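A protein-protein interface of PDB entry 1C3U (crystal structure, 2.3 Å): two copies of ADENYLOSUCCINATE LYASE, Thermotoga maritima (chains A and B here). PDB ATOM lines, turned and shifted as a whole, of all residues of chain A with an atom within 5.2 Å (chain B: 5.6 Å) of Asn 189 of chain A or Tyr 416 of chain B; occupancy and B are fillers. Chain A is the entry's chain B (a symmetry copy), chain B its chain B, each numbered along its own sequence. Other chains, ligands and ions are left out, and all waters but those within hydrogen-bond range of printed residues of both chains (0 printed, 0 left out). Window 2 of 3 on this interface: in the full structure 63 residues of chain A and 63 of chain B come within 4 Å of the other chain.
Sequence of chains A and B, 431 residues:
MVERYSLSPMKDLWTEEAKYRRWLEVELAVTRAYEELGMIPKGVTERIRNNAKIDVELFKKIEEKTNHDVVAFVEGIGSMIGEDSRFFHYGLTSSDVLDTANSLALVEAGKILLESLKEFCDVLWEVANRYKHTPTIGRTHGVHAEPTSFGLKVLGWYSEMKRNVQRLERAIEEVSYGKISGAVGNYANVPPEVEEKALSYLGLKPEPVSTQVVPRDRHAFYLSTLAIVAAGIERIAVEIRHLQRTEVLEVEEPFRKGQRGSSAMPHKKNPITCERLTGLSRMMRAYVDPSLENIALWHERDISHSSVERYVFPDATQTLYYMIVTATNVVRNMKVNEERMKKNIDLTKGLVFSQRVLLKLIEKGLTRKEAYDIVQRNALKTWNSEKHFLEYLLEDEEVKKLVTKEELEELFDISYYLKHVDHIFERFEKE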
ATOM      1  N   TYR A  34      32.765 -18.166  15.156  1.00  0.00           N
ATOM      2  CA  TYR A  34      33.178 -16.919  14.516  1.00  0.00           C
ATOM      3  C   TYR A  34      34.367 -17.087  13.557  1.00  0.00           C
ATOM      4  O   TYR A  34      34.362 -16.490  12.488  1.00  0.00           O
ATOM      5  CB  TYR A  34      33.627 -15.881  15.548  1.00  0.00           C
ATOM      6  CG  TYR A  34      32.577 -15.066  16.240  1.00  0.00           C
ATOM      7  CD1 TYR A  34      32.339 -15.127  17.608  1.00  0.00           C
ATOM      8  CD2 TYR A  34      31.788 -14.189  15.504  1.00  0.00           C
ATOM      9  CE1 TYR A  34      31.389 -14.356  18.239  1.00  0.00           C
ATOM     10  CE2 TYR A  34      30.831 -13.403  16.083  1.00  0.00           C
ATOM     11  CZ  TYR A  34      30.648 -13.487  17.469  1.00  0.00           C
ATOM     12  OH  TYR A  34      29.680 -12.655  18.012  1.00  0.00           O
ATOM     13  N   TYR A  90      32.023 -12.568  22.774  1.00  0.00           N
ATOM     14  CA  TYR A  90      31.798 -11.430  21.912  1.00  0.00           C
ATOM     15  C   TYR A  90      30.352 -11.368  21.461  1.00  0.00           C
ATOM     16  O   TYR A  90      29.841 -12.221  20.705  1.00  0.00           O
ATOM     17  CB  TYR A  90      32.822 -11.495  20.759  1.00  0.00           C
ATOM     18  CG  TYR A  90      32.732 -10.219  19.948  1.00  0.00           C
ATOM     19  CD1 TYR A  90      32.178 -10.231  18.696  1.00  0.00           C
ATOM     20  CD2 TYR A  90      33.184  -9.017  20.467  1.00  0.00           C
ATOM     21  CE1 TYR A  90      32.097  -9.048  17.968  1.00  0.00           C
ATOM     22  CE2 TYR A  90      33.093  -7.832  19.766  1.00  0.00           C
ATOM     23  CZ  TYR A  90      32.546  -7.857  18.513  1.00  0.00           C
ATOM     24  OH  TYR A  90      32.425  -6.702  17.754  1.00  0.00           O
ATOM     25  N   GLY A  91      29.655 -10.335  21.943  1.00  0.00           N
ATOM     26  CA  GLY A  91      28.237 -10.211  21.700  1.00  0.00           C
ATOM     27  C   GLY A  91      27.367 -11.008  22.653  1.00  0.00           C
ATOM     28  O   GLY A  91      26.139 -10.883  22.590  1.00  0.00           O
ATOM     29  N   ALA A 183      21.515 -10.557  24.265  1.00  0.00           N
ATOM     30  CA  ALA A 183      20.778 -10.021  25.392  1.00  0.00           C
ATOM     31  C   ALA A 183      19.316 -10.410  25.420  1.00  0.00           C
ATOM     32  O   ALA A 183      18.870 -10.788  26.528  1.00  0.00           O
ATOM     33  CB  ALA A 183      20.893  -8.496  25.456  1.00  0.00           C
ATOM     34  N   TYR A 187      19.555 -12.077  18.323  1.00  0.00           N
ATOM     35  CA  TYR A 187      20.771 -12.053  17.515  1.00  0.00           C
ATOM     36  C   TYR A 187      21.222 -10.643  17.154  1.00  0.00           C
ATOM     37  O   TYR A 187      22.143 -10.471  16.333  1.00  0.00           O
ATOM     38  CB  TYR A 187      20.697 -13.000  16.293  1.00  0.00           C
ATOM     39  CG  TYR A 187      20.171 -14.366  16.686  1.00  0.00           C
ATOM     40  CD1 TYR A 187      18.830 -14.696  16.506  1.00  0.00           C
ATOM     41  CD2 TYR A 187      20.975 -15.318  17.284  1.00  0.00           C
ATOM     42  CE1 TYR A 187      18.289 -15.926  16.896  1.00  0.00           C
ATOM     43  CE2 TYR A 187      20.486 -16.552  17.645  1.00  0.00           C
ATOM     44  CZ  TYR A 187      19.153 -16.839  17.460  1.00  0.00           C
ATOM     45  OH  TYR A 187      18.681 -18.078  17.831  1.00  0.00           O
ATOM     46  N   ALA A 188      20.761  -9.609  17.878  1.00  0.00           N
ATOM     47  CA  ALA A 188      21.209  -8.253  17.578  1.00  0.00           C
ATOM     48  C   ALA A 188      22.737  -8.179  17.705  1.00  0.00           C
ATOM     49  O   ALA A 188      23.309  -7.544  16.824  1.00  0.00           O
ATOM     50  CB  ALA A 188      20.531  -7.243  18.467  1.00  0.00           C
ATOM     51  N   ASN A 189      23.359  -8.796  18.710  1.00  0.00           N
ATOM     52  CA  ASN A 189      24.778  -8.640  18.964  1.00  0.00           C
ATOM     53  C   ASN A 189      25.633  -9.835  18.544  1.00  0.00           C
ATOM     54  O   ASN A 189      26.866  -9.775  18.639  1.00  0.00           O
ATOM     55  CB  ASN A 189      24.998  -8.370  20.496  1.00  0.00           C
ATOM     56  CG  ASN A 189      24.072  -7.239  20.942  1.00  0.00           C
ATOM     57  OD1 ASN A 189      24.025  -6.221  20.240  1.00  0.00           O
ATOM     58  ND2 ASN A 189      23.312  -7.295  22.028  1.00  0.00           N
ATOM     59  N   VAL A 190      25.018 -10.936  18.148  1.00  0.00           N
ATOM     60  CA  VAL A 190      25.708 -12.152  17.770  1.00  0.00           C
ATOM     61  C   VAL A 190      24.850 -12.899  16.740  1.00  0.00           C
ATOM     62  O   VAL A 190      23.717 -13.295  16.974  1.00  0.00           O
ATOM     63  CB  VAL A 190      26.049 -13.051  18.979  1.00  0.00           C
ATOM     64  CG1 VAL A 190      24.781 -13.278  19.814  1.00  0.00           C
ATOM     65  CG2 VAL A 190      26.644 -14.399  18.557  1.00  0.00           C
ATOM     66  N   PRO A 191      25.377 -13.107  15.539  1.00  0.00           N
ATOM     67  CA  PRO A 191      24.628 -13.682  14.424  1.00  0.00           C
ATOM     68  C   PRO A 191      24.198 -15.105  14.743  1.00  0.00           C
ATOM     69  O   PRO A 191      24.856 -15.884  15.437  1.00  0.00           O
ATOM     70  CB  PRO A 191      25.587 -13.669  13.246  1.00  0.00           C
ATOM     71  CG  PRO A 191      26.852 -13.070  13.708  1.00  0.00           C
ATOM     72  CD  PRO A 191      26.826 -12.942  15.215  1.00  0.00           C
ATOM     73  N   GLU B 146      16.854  -4.283  25.501  1.00  0.00           N
ATOM     74  CA  GLU B 146      17.129  -3.880  24.112  1.00  0.00           C
ATOM     75  C   GLU B 146      15.827  -4.015  23.322  1.00  0.00           C
ATOM     76  O   GLU B 146      14.993  -4.799  23.749  1.00  0.00           O
ATOM     77  CB  GLU B 146      18.162  -4.809  23.456  1.00  0.00           C
ATOM     78  CG  GLU B 146      19.553  -4.674  24.026  1.00  0.00           C
ATOM     79  CD  GLU B 146      20.631  -5.489  23.362  1.00  0.00           C
ATOM     80  OE1 GLU B 146      20.371  -6.451  22.603  1.00  0.00           O
ATOM     81  OE2 GLU B 146      21.796  -5.120  23.626  1.00  0.00           O
ATOM     82  N   ARG B 356      25.678   0.204  22.540  1.00  0.00           N
ATOM     83  CA  ARG B 356      26.175   0.465  21.193  1.00  0.00           C
ATOM     84  C   ARG B 356      27.157   1.637  21.223  1.00  0.00           C
ATOM     85  O   ARG B 356      28.288   1.560  20.752  1.00  0.00           O
ATOM     86  CB  ARG B 356      25.012   0.745  20.241  1.00  0.00           C
ATOM     87  CG  ARG B 356      24.092  -0.449  19.993  1.00  0.00           C
ATOM     88  CD  ARG B 356      23.459  -0.351  18.598  1.00  0.00           C
ATOM     89  NE  ARG B 356      24.483  -0.582  17.596  1.00  0.00           N
ATOM     90  CZ  ARG B 356      24.502  -0.298  16.305  1.00  0.00           C
ATOM     91  NH1 ARG B 356      25.564  -0.596  15.558  1.00  0.00           N
ATOM     92  NH2 ARG B 356      23.473   0.269  15.700  1.00  0.00           N
ATOM     93  N   ASP B 413      19.469   3.461  15.591  1.00  0.00           N
ATOM     94  CA  ASP B 413      18.572   2.792  14.634  1.00  0.00           C
ATOM     95  C   ASP B 413      18.022   1.533  15.302  1.00  0.00           C
ATOM     96  O   ASP B 413      18.734   0.627  15.751  1.00  0.00           O
ATOM     97  CB  ASP B 413      19.352   2.394  13.405  1.00  0.00           C
ATOM     98  CG  ASP B 413      18.747   2.417  12.032  1.00  0.00           C
ATOM     99  OD1 ASP B 413      17.523   2.175  11.788  1.00  0.00           O
ATOM    100  OD2 ASP B 413      19.588   2.667  11.099  1.00  0.00           O
ATOM    101  N   ILE B 414      16.725   1.399  15.366  1.00  0.00           N
ATOM    102  CA  ILE B 414      16.043   0.211  15.841  1.00  0.00           C
ATOM    103  C   ILE B 414      16.200  -1.013  14.970  1.00  0.00           C
ATOM    104  O   ILE B 414      16.232  -2.154  15.485  1.00  0.00           O
ATOM    105  CB  ILE B 414      14.589   0.719  15.989  1.00  0.00           C
ATOM    106  CG1 ILE B 414      13.813  -0.152  16.936  1.00  0.00           C
ATOM    107  CG2 ILE B 414      13.984   0.801  14.589  1.00  0.00           C
ATOM    108  CD1 ILE B 414      13.014  -1.279  16.356  1.00  0.00           C
ATOM    109  N   SER B 415      16.409  -0.776  13.668  1.00  0.00           N
ATOM    110  CA  SER B 415      16.609  -1.836  12.712  1.00  0.00           C
ATOM    111  C   SER B 415      17.838  -2.633  13.128  1.00  0.00           C
ATOM    112  O   SER B 415      17.740  -3.789  12.736  1.00  0.00           O
ATOM    113  CB  SER B 415      16.804  -1.405  11.240  1.00  0.00           C
ATOM    114  OG  SER B 415      17.765  -0.353  11.240  1.00  0.00           O
ATOM    115  N   TYR B 416      18.838  -2.178  13.833  1.00  0.00           N
ATOM    116  CA  TYR B 416      19.935  -3.045  14.281  1.00  0.00           C
ATOM    117  C   TYR B 416      19.470  -4.266  15.073  1.00  0.00           C
ATOM    118  O   TYR B 416      19.885  -5.430  14.902  1.00  0.00           O
ATOM    119  CB  TYR B 416      20.872  -2.216  15.169  1.00  0.00           C
ATOM    120  CG  TYR B 416      22.004  -2.932  15.865  1.00  0.00           C
ATOM    121  CD1 TYR B 416      23.273  -3.095  15.315  1.00  0.00           C
ATOM    122  CD2 TYR B 416      21.761  -3.474  17.124  1.00  0.00           C
ATOM    123  CE1 TYR B 416      24.285  -3.743  16.011  1.00  0.00           C
ATOM    124  CE2 TYR B 416      22.762  -4.148  17.814  1.00  0.00           C
ATOM    125  CZ  TYR B 416      24.011  -4.268  17.250  1.00  0.00           C
ATOM    126  OH  TYR B 416      24.982  -4.935  17.966  1.00  0.00           O
ATOM    127  N   TYR B 417      18.397  -4.103  15.875  1.00  0.00           N
ATOM    128  CA  TYR B 417      17.990  -5.048  16.904  1.00  0.00           C
ATOM    129  C   TYR B 417      17.120  -5.982  16.192  1.00  0.00           C
ATOM    130  O   TYR B 417      17.046  -7.174  16.501  1.00  0.00           O
ATOM    131  CB  TYR B 417      17.183  -4.322  17.989  1.00  0.00           C
ATOM    132  CG  TYR B 417      18.229  -3.581  18.775  1.00  0.00           C
ATOM    133  CD1 TYR B 417      18.488  -2.239  18.543  1.00  0.00           C
ATOM    134  CD2 TYR B 417      19.014  -4.262  19.693  1.00  0.00           C
ATOM    135  CE1 TYR B 417      19.498  -1.586  19.225  1.00  0.00           C
ATOM    136  CE2 TYR B 417      20.025  -3.619  20.380  1.00  0.00           C
ATOM    137  CZ  TYR B 417      20.262  -2.281  20.142  1.00  0.00           C
ATOM    138  OH  TYR B 417      21.269  -1.636  20.824  1.00  0.00           O
ATOM    139  N   LEU B 418      16.452  -5.345  15.277  1.00  0.00           N
ATOM    140  CA  LEU B 418      15.847  -6.076  14.283  1.00  0.00           C
ATOM    141  C   LEU B 418      16.232  -6.738  12.925  1.00  0.00           C
ATOM    142  O   LEU B 418      15.282  -7.109  12.175  1.00  0.00           O
ATOM    143  CB  LEU B 418      14.689  -5.226  13.741  1.00  0.00           C
ATOM    144  CG  LEU B 418      13.661  -4.776  14.792  1.00  0.00           C
ATOM    145  CD1 LEU B 418      12.353  -4.358  14.140  1.00  0.00           C
ATOM    146  CD2 LEU B 418      13.409  -5.881  15.815  1.00  0.00           C
ATOM    147  N   LYS B 419      17.465  -6.932  12.605  1.00  0.00           N
ATOM    148  CA  LYS B 419      17.952  -7.629  11.364  1.00  0.00           C
ATOM    149  C   LYS B 419      17.734  -9.133  11.275  1.00  0.00           C
ATOM    150  O   LYS B 419      17.729  -9.687  10.120  1.00  0.00           O
ATOM    151  CB  LYS B 419      19.452  -7.397  11.211  1.00  0.00           C
ATOM    152  CG  LYS B 419      20.254  -7.606  12.491  1.00  0.00           C
ATOM    153  CD  LYS B 419      21.733  -7.396  12.223  1.00  0.00           C
ATOM    154  CE  LYS B 419      22.556  -7.573  13.481  1.00  0.00           C
ATOM    155  NZ  LYS B 419      22.271  -6.508  14.481  1.00  0.00           N
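Among the printed residues, merely in contact across the chains: Ala 183 of chain A with Glu 146 of chain B (3.5 Å) and Ala 188 of chain A with Tyr 417 of chain B (3.6 Å).
OE2 of Glu 146 of chain B lies within hydrogen-bond range of ND2 of Asn 189 of chain A, at 3.1 Å. The backbone carbonyl oxygen of Ala 188 of chain A is in hydrogen-bond range of the side-chain hydroxyl of Tyr 416 of chain B. The side-chain amide oxygen (OD1) of Asn 189 of chain A sits at hydrogen-bond distance from the side-chain hydroxyl (OH) of Tyr 416 of chain B. The side-chain amino group (NZ) of Lys 419 of chain B lies within hydrogen-bond range of the backbone carbonyl oxygen (O) of Ala 188 of chain A, at 2.8 Å.
Asn 189 of chain A touches just these residues of chain B: Glu 146 (3.1 Å) and Tyr 416 (2.8 Å). Tyr 416 of chain B touches just these residues of chain A: Ala 188 and Asn 189. Of the printed residues of chain A, Tyr 417 of chain B touches Ala 188. Printed residues of chain A within 4 Å of Lys 419 of chain B: Ala 188. Printed residues of chain B within 4 Å of Ala 183 of chain A: Glu 146 (3.5 Å). Printed residues of chain A within 4 Å of Glu 146 of chain B: Ala 183 (3.5 Å) and Asn 189 (3.1 Å). Val 190 of chain A touches none of the printed residues of chain B. The nearest residue of chain B that does not touch Asn 189 of chain A is Tyr 417 of chain B (4.8 Å). The nearest printed residue of chain A that does not touch Tyr 416 of chain B is Tyr 187 of chain A (5.7 Å). The nearest printed residue of chain A that does not touch Glu 146 of chain B is Ala 188 of chain A (4.2 Å).
No position is printed for both chains.
Printed residues of chain B that touch a printed residue of chain A: Glu 146, Tyr 416, Tyr 417 and Lys 419. Hydrophobic or aromatic side chains of chain B within 4 Å of the printed part of chain A: Tyr 416 and Tyr 417. Among the printed residues, 6 pairs touch across the chains. Among the printed residues, no Asp or Glu carboxylate lies within 4 Å of a Lys or Arg side-chain nitrogen of the other chain.
The backbone carbonyl oxygen of Tyr 416 of chain B lies within hydrogen-bond range of the side-chain amino group of Lys 419 of chain B (2.7 Å).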
